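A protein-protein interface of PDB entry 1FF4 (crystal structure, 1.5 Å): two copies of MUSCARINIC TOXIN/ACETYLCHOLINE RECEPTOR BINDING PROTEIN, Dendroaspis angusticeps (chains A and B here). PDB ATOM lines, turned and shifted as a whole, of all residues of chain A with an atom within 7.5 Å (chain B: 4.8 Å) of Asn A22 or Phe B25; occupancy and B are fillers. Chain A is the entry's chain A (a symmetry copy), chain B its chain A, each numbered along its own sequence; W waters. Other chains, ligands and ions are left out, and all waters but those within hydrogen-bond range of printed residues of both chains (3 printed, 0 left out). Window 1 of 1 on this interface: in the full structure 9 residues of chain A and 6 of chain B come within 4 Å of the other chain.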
ATOM      1  N   LEU A   1      -0.929   4.975  -4.591  1.00  0.00           N
ATOM      2  CA  LEU A   1      -1.007   3.654  -3.904  1.00  0.00           C
ATOM      3  C   LEU A   1      -0.442   2.576  -4.843  1.00  0.00           C
ATOM      4  O   LEU A   1      -0.609   2.630  -6.061  1.00  0.00           O
ATOM      5  CB  LEU A   1      -2.454   3.338  -3.501  1.00  0.00           C
ATOM      6  CG  LEU A   1      -2.742   2.027  -2.749  1.00  0.00           C
ATOM      7  CD1 LEU A   1      -2.206   2.084  -1.327  1.00  0.00           C
ATOM      8  CD2 LEU A   1      -4.228   1.811  -2.698  1.00  0.00           C
ATOM      9  N   CYS A   3      -0.211  -1.455  -5.261  1.00  0.00           N
ATOM     10  CA  CYS A   3      -0.796  -2.696  -4.807  1.00  0.00           C
ATOM     11  C   CYS A   3      -0.144  -3.856  -5.486  1.00  0.00           C
ATOM     12  O   CYS A   3       0.390  -3.734  -6.579  1.00  0.00           O
ATOM     13  CB  CYS A   3      -2.281  -2.754  -5.159  1.00  0.00           C
ATOM     14  SG  CYS A   3      -3.311  -1.456  -4.439  1.00  0.00           S
ATOM     15  N   CYS A  17      -1.736   2.293  -8.557  1.00  0.00           N
ATOM     16  CA  CYS A  17      -3.119   2.375  -8.924  1.00  0.00           C
ATOM     17  C   CYS A  17      -3.387   3.666  -9.649  1.00  0.00           C
ATOM     18  O   CYS A  17      -2.755   4.680  -9.394  1.00  0.00           O
ATOM     19  CB  CYS A  17      -3.988   2.311  -7.684  1.00  0.00           C
ATOM     20  SG  CYS A  17      -3.648   0.824  -6.725  1.00  0.00           S
ATOM     21  N   PRO A  18      -4.308   3.630 -10.610  1.00  0.00           N
ATOM     22  CA  PRO A  18      -4.647   4.842 -11.350  1.00  0.00           C
ATOM     23  C   PRO A  18      -5.259   5.833 -10.337  1.00  0.00           C
ATOM     24  O   PRO A  18      -5.738   5.419  -9.272  1.00  0.00           O
ATOM     25  CB  PRO A  18      -5.726   4.349 -12.325  1.00  0.00           C
ATOM     26  CG  PRO A  18      -5.513   2.868 -12.412  1.00  0.00           C
ATOM     27  CD  PRO A  18      -5.088   2.462 -11.065  1.00  0.00           C
ATOM     28  N   ALA A  19      -5.219   7.128 -10.650  1.00  0.00           N
ATOM     29  CA  ALA A  19      -5.801   8.153  -9.786  1.00  0.00           C
ATOM     30  C   ALA A  19      -7.268   7.811  -9.525  1.00  0.00           C
ATOM     31  O   ALA A  19      -7.984   7.507 -10.474  1.00  0.00           O
ATOM     32  CB  ALA A  19      -5.722   9.506 -10.476  1.00  0.00           C
ATOM     33  N   GLY A  20      -7.705   7.859  -8.260  1.00  0.00           N
ATOM     34  CA  GLY A  20      -9.081   7.557  -7.901  1.00  0.00           C
ATOM     35  C   GLY A  20      -9.275   6.154  -7.352  1.00  0.00           C
ATOM     36  O   GLY A  20     -10.353   5.831  -6.872  1.00  0.00           O
ATOM     37  N   GLN A  21      -8.245   5.319  -7.461  1.00  0.00           N
ATOM     38  CA  GLN A  21      -8.264   3.948  -6.968  1.00  0.00           C
ATOM     39  C   GLN A  21      -7.337   3.852  -5.761  1.00  0.00           C
ATOM     40  O   GLN A  21      -6.131   3.665  -5.887  1.00  0.00           O
ATOM     41  CB  GLN A  21      -7.837   3.000  -8.079  1.00  0.00           C
ATOM     42  CG  GLN A  21      -8.876   2.925  -9.183  1.00  0.00           C
ATOM     43  CD  GLN A  21      -8.649   1.767 -10.122  1.00  0.00           C
ATOM     44  OE1 GLN A  21      -7.836   0.893  -9.872  1.00  0.00           O
ATOM     45  NE2 GLN A  21      -9.384   1.752 -11.208  1.00  0.00           N
ATOM     46  N   ASN A  22      -7.932   3.938  -4.587  1.00  0.00           N
ATOM     47  CA  ASN A  22      -7.183   3.942  -3.354  1.00  0.00           C
ATOM     48  C   ASN A  22      -7.348   2.711  -2.500  1.00  0.00           C
ATOM     49  O   ASN A  22      -7.047   2.728  -1.317  1.00  0.00           O
ATOM     50  CB  ASN A  22      -7.575   5.181  -2.558  1.00  0.00           C
ATOM     51  CG  ASN A  22      -7.042   6.447  -3.184  1.00  0.00           C
ATOM     52  OD1 ASN A  22      -5.997   6.430  -3.828  1.00  0.00           O
ATOM     53  ND2 ASN A  22      -7.751   7.545  -3.004  1.00  0.00           N
ATOM     54  N   VAL A  23      -7.780   1.618  -3.107  1.00  0.00           N
ATOM     55  CA  VAL A  23      -7.957   0.388  -2.354  1.00  0.00           C
ATOM     56  C   VAL A  23      -7.178  -0.730  -3.028  1.00  0.00           C
ATOM     57  O   VAL A  23      -7.112  -0.793  -4.258  1.00  0.00           O
ATOM     58  CB  VAL A  23      -9.462  -0.032  -2.318  1.00  0.00           C
ATOM     59  CG1 VAL A  23      -9.662  -1.348  -1.558  1.00  0.00           C
ATOM     60  CG2 VAL A  23     -10.313   1.086  -1.754  1.00  0.00           C
ATOM     61  N   CYS A  24      -6.463  -1.505  -2.221  1.00  0.00           N
ATOM     62  CA  CYS A  24      -5.795  -2.716  -2.714  1.00  0.00           C
ATOM     63  C   CYS A  24      -6.711  -3.824  -2.216  1.00  0.00           C
ATOM     64  O   CYS A  24      -7.278  -3.729  -1.138  1.00  0.00           O
ATOM     65  CB  CYS A  24      -4.453  -2.976  -2.055  1.00  0.00           C
ATOM     66  SG  CYS A  24      -3.177  -1.763  -2.439  1.00  0.00           S
ATOM     67  N   CYS A  42      -5.648  -3.231  -7.698  1.00  0.00           N
ATOM     68  CA  CYS A  42      -6.169  -1.911  -7.353  1.00  0.00           C
ATOM     69  C   CYS A  42      -7.658  -1.879  -7.603  1.00  0.00           C
ATOM     70  O   CYS A  42      -8.141  -2.546  -8.498  1.00  0.00           O
ATOM     71  CB  CYS A  42      -5.562  -0.866  -8.289  1.00  0.00           C
ATOM     72  SG  CYS A  42      -3.772  -0.652  -8.110  1.00  0.00           S
ATOM     73  N   ALA A  43      -8.373  -1.051  -6.858  1.00  0.00           N
ATOM     74  CA  ALA A  43      -9.803  -0.878  -7.056  1.00  0.00           C
ATOM     75  C   ALA A  43     -10.209   0.485  -6.490  1.00  0.00           C
ATOM     76  O   ALA A  43      -9.494   1.052  -5.664  1.00  0.00           O
ATOM     77  CB  ALA A  43     -10.573  -1.981  -6.376  1.00  0.00           C
ATOM     78  N   ALA A  44     -11.343   1.006  -6.948  1.00  0.00           N
ATOM     79  CA  ALA A  44     -11.864   2.288  -6.479  1.00  0.00           C
ATOM     80  C   ALA A  44     -12.547   2.089  -5.133  1.00  0.00           C
ATOM     81  O   ALA A  44     -12.583   2.983  -4.288  1.00  0.00           O
ATOM     82  CB  ALA A  44     -12.849   2.846  -7.477  1.00  0.00           C
ATOM     83  N   THR A  45     -13.120   0.906  -4.954  1.00  0.00           N
ATOM     84  CA  THR A  45     -13.803   0.557  -3.712  1.00  0.00           C
ATOM     85  C   THR A  45     -13.493  -0.907  -3.486  1.00  0.00           C
ATOM     86  O   THR A  45     -13.085  -1.601  -4.408  1.00  0.00           O
ATOM     87  CB  THR A  45     -15.318   0.642  -3.918  1.00  0.00           C
ATOM     88  OG1 THR A  45     -15.652  -0.090  -5.114  1.00  0.00           O
ATOM     89  CG2 THR A  45     -15.793   2.060  -4.023  1.00  0.00           C
ATOM     90  N   CYS A  58      -7.615  -3.007   1.690  1.00  0.00           N
ATOM     91  CA  CYS A  58      -6.802  -2.144   2.511  1.00  0.00           C
ATOM     92  C   CYS A  58      -6.296  -0.976   1.684  1.00  0.00           C
ATOM     93  O   CYS A  58      -6.345  -1.000   0.455  1.00  0.00           O
ATOM     94  CB  CYS A  58      -5.678  -2.962   3.119  1.00  0.00           C
ATOM     95  SG  CYS A  58      -4.795  -3.941   1.880  1.00  0.00           S
ATOM     96  N   GLY A  59      -5.836   0.062   2.372  1.00  0.00           N
ATOM     97  CA  GLY A  59      -5.400   1.241   1.665  1.00  0.00           C
ATOM     98  C   GLY A  59      -3.963   1.645   1.806  1.00  0.00           C
ATOM     99  O   GLY A  59      -3.660   2.802   1.580  1.00  0.00           O
ATOM    100  N   THR A  60      -3.076   0.725   2.158  1.00  0.00           N
ATOM    101  CA  THR A  60      -1.664   1.063   2.264  1.00  0.00           C
ATOM    102  C   THR A  60      -0.865   0.266   1.252  1.00  0.00           C
ATOM    103  O   THR A  60      -1.291  -0.801   0.827  1.00  0.00           O
ATOM    104  CB  THR A  60      -1.115   0.878   3.694  1.00  0.00           C
ATOM    105  OG1 THR A  60      -1.303  -0.470   4.128  1.00  0.00           O
ATOM    106  CG2 THR A  60      -1.839   1.805   4.642  1.00  0.00           C
ATOM    107  N   CYS A  63      -0.387  -3.734   0.846  1.00  0.00           N
ATOM    108  CA  CYS A  63      -1.045  -4.291   2.017  1.00  0.00           C
ATOM    109  C   CYS A  63      -1.809  -5.559   1.652  1.00  0.00           C
ATOM    110  O   CYS A  63      -2.189  -6.322   2.538  1.00  0.00           O
ATOM    111  CB  CYS A  63      -2.000  -3.262   2.613  1.00  0.00           C
ATOM    112  SG  CYS A  63      -3.253  -2.713   1.417  1.00  0.00           S
ATOM    113  N   VAL B  23      -4.796  16.551  -5.002  1.00  0.00           N
ATOM    114  CA  VAL B  23      -6.184  16.676  -5.410  1.00  0.00           C
ATOM    115  C   VAL B  23      -7.052  15.814  -4.510  1.00  0.00           C
ATOM    116  O   VAL B  23      -6.647  14.717  -4.115  1.00  0.00           O
ATOM    117  CB  VAL B  23      -6.380  16.182  -6.880  1.00  0.00           C
ATOM    118  CG1 VAL B  23      -7.847  16.273  -7.315  1.00  0.00           C
ATOM    119  CG2 VAL B  23      -5.460  16.931  -7.821  1.00  0.00           C
ATOM    120  N   CYS B  24      -8.166  16.381  -4.062  1.00  0.00           N
ATOM    121  CA  CYS B  24      -9.173  15.614  -3.319  1.00  0.00           C
ATOM    122  C   CYS B  24     -10.254  15.387  -4.366  1.00  0.00           C
ATOM    123  O   CYS B  24     -10.504  16.243  -5.201  1.00  0.00           O
ATOM    124  CB  CYS B  24      -9.844  16.408  -2.213  1.00  0.00           C
ATOM    125  SG  CYS B  24      -8.759  16.862  -0.848  1.00  0.00           S
ATOM    126  N   PHE B  25     -10.906  14.242  -4.318  1.00  0.00           N
ATOM    127  CA  PHE B  25     -11.978  14.006  -5.256  1.00  0.00           C
ATOM    128  C   PHE B  25     -13.142  13.397  -4.513  1.00  0.00           C
ATOM    129  O   PHE B  25     -12.991  12.798  -3.456  1.00  0.00           O
ATOM    130  CB  PHE B  25     -11.545  13.095  -6.411  1.00  0.00           C
ATOM    131  CG  PHE B  25     -11.335  11.663  -6.004  1.00  0.00           C
ATOM    132  CD1 PHE B  25     -12.399  10.755  -6.008  1.00  0.00           C
ATOM    133  CD2 PHE B  25     -10.087  11.220  -5.591  1.00  0.00           C
ATOM    134  CE1 PHE B  25     -12.207   9.425  -5.597  1.00  0.00           C
ATOM    135  CE2 PHE B  25      -9.882   9.897  -5.178  1.00  0.00           C
ATOM    136  CZ  PHE B  25     -10.942   8.996  -5.179  1.00  0.00           C
ATOM    137  N   LYS B  26     -14.319  13.641  -5.064  1.00  0.00           N
ATOM    138  CA  LYS B  26     -15.561  13.086  -4.564  1.00  0.00           C
ATOM    139  C   LYS B  26     -16.245  12.642  -5.866  1.00  0.00           C
ATOM    140  O   LYS B  26     -16.496  13.452  -6.763  1.00  0.00           O
ATOM    141  CB  LYS B  26     -16.395  14.136  -3.846  1.00  0.00           C
ATOM    142  CG  LYS B  26     -17.704  13.600  -3.331  1.00  0.00           C
ATOM    143  CD  LYS B  26     -18.453  14.671  -2.573  1.00  0.00           C
ATOM    144  CE  LYS B  26     -19.755  14.152  -2.020  1.00  0.00           C
ATOM    145  NZ  LYS B  26     -20.448  15.282  -1.381  1.00  0.00           N
ATOM    146  N   ARG B  27     -16.429  11.333  -6.004  1.00  0.00           N
ATOM    147  CA  ARG B  27     -17.048  10.766  -7.192  1.00  0.00           C
ATOM    148  C   ARG B  27     -18.337  10.055  -6.788  1.00  0.00           C
ATOM    149  O   ARG B  27     -18.386   9.328  -5.788  1.00  0.00           O
ATOM    150  CB  ARG B  27     -16.092   9.781  -7.865  1.00  0.00           C
ATOM    151  CG  ARG B  27     -16.591   9.194  -9.170  1.00  0.00           C
ATOM    152  CD  ARG B  27     -15.620   8.146  -9.671  1.00  0.00           C
ATOM    153  NE  ARG B  27     -15.997   7.654 -11.000  1.00  0.00           N
ATOM    154  CZ  ARG B  27     -15.162   7.537 -12.042  1.00  0.00           C
ATOM    155  NH1 ARG B  27     -13.871   7.862 -11.915  1.00  0.00           N
ATOM    156  NH2 ARG B  27     -15.630   7.166 -13.235  1.00  0.00           N
ATOM    157  N   ILE B  39     -17.403   7.954  -3.622  1.00  0.00           N
ATOM    158  CA  ILE B  39     -16.027   7.578  -3.344  1.00  0.00           C
ATOM    159  C   ILE B  39     -15.269   8.891  -3.142  1.00  0.00           C
ATOM    160  O   ILE B  39     -15.382   9.799  -3.946  1.00  0.00           O
ATOM    161  CB  ILE B  39     -15.428   6.816  -4.536  1.00  0.00           C
ATOM    162  CG1 ILE B  39     -16.331   5.631  -4.904  1.00  0.00           C
ATOM    163  CG2 ILE B  39     -14.005   6.338  -4.214  1.00  0.00           C
ATOM    164  CD1 ILE B  39     -16.092   5.155  -6.308  1.00  0.00           C
ATOM    165  N   LYS B  40     -14.501   8.967  -2.067  1.00  0.00           N
ATOM    166  CA  LYS B  40     -13.740  10.163  -1.762  1.00  0.00           C
ATOM    167  C   LYS B  40     -12.310   9.801  -1.406  1.00  0.00           C
ATOM    168  O   LYS B  40     -12.036   8.747  -0.832  1.00  0.00           O
ATOM    169  CB  LYS B  40     -14.349  10.880  -0.567  1.00  0.00           C
ATOM    170  CG  LYS B  40     -15.760  11.317  -0.737  1.00  0.00           C
ATOM    171  CD  LYS B  40     -16.295  11.651   0.630  1.00  0.00           C
ATOM    172  CE  LYS B  40     -17.701  12.132   0.569  1.00  0.00           C
ATOM    173  NZ  LYS B  40     -18.230  12.308   1.946  1.00  0.00           N
ATOM    174  N   GLY B  41     -11.398  10.712  -1.718  1.00  0.00           N
ATOM    175  CA  GLY B  41     -10.017  10.474  -1.365  1.00  0.00           C
ATOM    176  C   GLY B  41      -9.023  11.401  -2.004  1.00  0.00           C
ATOM    177  O   GLY B  41      -9.391  12.372  -2.643  1.00  0.00           O
ATOM    178  N   CYS B  42      -7.754  11.039  -1.843  1.00  0.00           N
ATOM    179  CA  CYS B  42      -6.610  11.754  -2.400  1.00  0.00           C
ATOM    180  C   CYS B  42      -6.285  11.194  -3.765  1.00  0.00           C
ATOM    181  O   CYS B  42      -6.486  10.018  -4.006  1.00  0.00           O
ATOM    182  CB  CYS B  42      -5.378  11.495  -1.534  1.00  0.00           C
ATOM    183  SG  CYS B  42      -5.490  12.163   0.146  1.00  0.00           S
ATOM    184  N   ALA B  43      -5.718  12.018  -4.631  1.00  0.00           N
ATOM    185  CA  ALA B  43      -5.292  11.574  -5.948  1.00  0.00           C
ATOM    186  C   ALA B  43      -4.208  12.530  -6.455  1.00  0.00           C
ATOM    187  O   ALA B  43      -4.103  13.658  -5.974  1.00  0.00           O
ATOM    188  CB  ALA B  43      -6.457  11.546  -6.904  1.00  0.00           C
ATOM    189  N   PRO B  47      -9.341  12.069 -11.080  1.00  0.00           N
ATOM    190  CA  PRO B  47      -9.591  10.774 -11.734  1.00  0.00           C
ATOM    191  C   PRO B  47     -10.323  10.915 -13.055  1.00  0.00           C
ATOM    192  O   PRO B  47     -11.222  11.755 -13.202  1.00  0.00           O
ATOM    193  CB  PRO B  47     -10.463  10.043 -10.716  1.00  0.00           C
ATOM    194  CG  PRO B  47      -9.976  10.568  -9.424  1.00  0.00           C
ATOM    195  CD  PRO B  47      -9.851  12.055  -9.699  1.00  0.00           C
ATOM    196  N   ILE B  55     -18.189  14.097 -10.824  1.00  0.00           N
ATOM    197  CA  ILE B  55     -16.987  14.045 -10.026  1.00  0.00           C
ATOM    198  C   ILE B  55     -16.658  15.460  -9.635  1.00  0.00           C
ATOM    199  O   ILE B  55     -16.910  16.402 -10.378  1.00  0.00           O
ATOM    200  CB  ILE B  55     -15.792  13.375 -10.789  1.00  0.00           C
ATOM    201  CG1 ILE B  55     -14.603  13.144  -9.847  1.00  0.00           C
ATOM    202  CG2 ILE B  55     -15.374  14.214 -11.961  1.00  0.00           C
ATOM    203  CD1 ILE B  55     -13.583  12.177 -10.377  1.00  0.00           C
ATOM    204  N   ARG B  56     -16.138  15.579  -8.429  1.00  0.00           N
ATOM    205  CA  ARG B  56     -15.719  16.840  -7.858  1.00  0.00           C
ATOM    206  C   ARG B  56     -14.234  16.700  -7.532  1.00  0.00           C
ATOM    207  O   ARG B  56     -13.842  15.785  -6.833  1.00  0.00           O
ATOM    208  CB  ARG B  56     -16.539  17.071  -6.592  1.00  0.00           C
ATOM    209  CG  ARG B  56     -15.910  17.962  -5.564  1.00  0.00           C
ATOM    210  CD  ARG B  56     -16.021  19.374  -5.956  1.00  0.00           C
ATOM    211  NE  ARG B  56     -15.588  20.170  -4.813  1.00  0.00           N
ATOM    212  CZ  ARG B  56     -15.439  21.487  -4.836  1.00  0.00           C
ATOM    213  NH1 ARG B  56     -15.028  22.108  -3.737  1.00  0.00           N
ATOM    214  NH2 ARG B  56     -15.730  22.169  -5.947  1.00  0.00           N
ATOM    215  N   CYS B  57     -13.412  17.559  -8.119  1.00  0.00           N
ATOM    216  CA  CYS B  57     -11.979  17.549  -7.857  1.00  0.00           C
ATOM    217  C   CYS B  57     -11.629  18.914  -7.353  1.00  0.00           C
ATOM    218  O   CYS B  57     -12.046  19.914  -7.924  1.00  0.00           O
ATOM    219  CB  CYS B  57     -11.179  17.243  -9.112  1.00  0.00           C
ATOM    220  SG  CYS B  57     -11.311  15.472  -9.480  1.00  0.00           S
ATOM    221  N   ASN B  64     -13.639  17.979  -0.593  1.00  0.00           N
ATOM    222  CA  ASN B  64     -14.390  16.862  -1.193  1.00  0.00           C
ATOM    223  C   ASN B  64     -15.356  16.225  -0.213  1.00  0.00           C
ATOM    224  O   ASN B  64     -15.599  15.023  -0.275  1.00  0.00           O
ATOM    225  CB  ASN B  64     -13.428  15.779  -1.701  1.00  0.00           C
ATOM    226  CG  ASN B  64     -12.659  15.086  -0.569  1.00  0.00           C
ATOM    227  OD1 ASN B  64     -12.426  15.671   0.492  1.00  0.00           O
ATOM    228  ND2 ASN B  64     -12.269  13.841  -0.792  1.00  0.00           N
HETATM  229  O   HOH W   1     -10.438   6.825  -1.862  1.00  0.00           O
HETATM  230  O   HOH W   2      -7.249   9.074  -0.094  1.00  0.00           O
HETATM  231  O   HOH W   3      -5.879   8.243  -6.223  1.00  0.00           O
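O of Cys B42 sits at hydrogen-bond distance from ND2 of Asn A22.
The backbone carbonyl oxygen (O) of Phe B25 lies within hydrogen-bond range of the side-chain amide nitrogen (ND2) of Asn B64, at 3.0 Å. The backbone NH (N) of Asn A22 is in hydrogen-bond range of the backbone carbonyl oxygen (O) of Ala A43 (3.5 Å). O of Gly B41 lies within hydrogen-bond range of N of Phe B25, 2.9 Å away. The side-chain sulfur (SG) of Cys A17 is disulfide-bonded to the side-chain sulfur (SG) of Cys A42, 2.0 Å away. SG of Cys A58 forms a disulfide with SG of Cys A63, 2.0 Å away. The backbone carbonyl oxygen (O) of Arg B27 lies within hydrogen-bond range of the backbone NH (N) of Ile B39 (2.7 Å).
Pro B47 touches Ala A19. CA of Gly A20 touches CZ of Phe B25, 3.6 Å away. Pro B47 touches Gly A20 (CG to CA, 3.5 Å). CE2 of Phe B25 touches ND2 of Asn A22 (3.8 Å). Ile B39 touches Ala A44. Ile B39 touches Thr A45.
Printed residues of chain B within 4 Å of Gly A20: Phe B25 and Pro B47. Of chain B, only Phe B25 and Cys B42 come within 4 Å of Asn A22. Ala A43 touches none of the printed residues of chain B. Of the printed residues of chain B, Thr A45 touches Ile B39. Phe B25 touches just these residues of chain A: Gly A20 (3.6 Å) and Asn A22 (3.8 Å). Printed residues of chain A within 4 Å of Ile B39: Ala A44 (3.6 Å) and Thr A45 (3.7 Å). Of the printed residues of chain A, Cys B42 touches Asn A22 (3.0 Å). The nearest residue of chain B that does not touch Asn A22 is Gly B41 (4.05 Å). The nearest printed residue of chain A that does not touch Pro B47 is Gln A21 (5.9 Å).
Printed residues of chain A that touch a printed residue of chain B: Ala A19, Gly A20, Asn A22, Ala A44 and Thr A45. Among the printed residues, 7 pairs touch across the chains. Among the printed residues, no Asp or Glu carboxylate lies within 4 Å of a Lys or Arg side-chain nitrogen of the other chain.
Positions printed for both chains: 23, 24, 42 and 43.
Water W2 bridges the backbone NH (N) of Cys B42 (2.7 Å) and the side-chain amide nitrogen (ND2) of Asn A22 (3.3 Å). Water W1 lies within hydrogen-bond range of O of Lys B40 (2.7 Å) and ND2 of Asn A22 (3.0 Å). Water W3 lies within hydrogen-bond range of the backbone NH (N) of Gly A20 (2.8 Å), the backbone carbonyl oxygen (O) of Cys B42 (2.9 Å) and the side-chain amide oxygen (OD1) of Asn A22 (3.0 Å).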
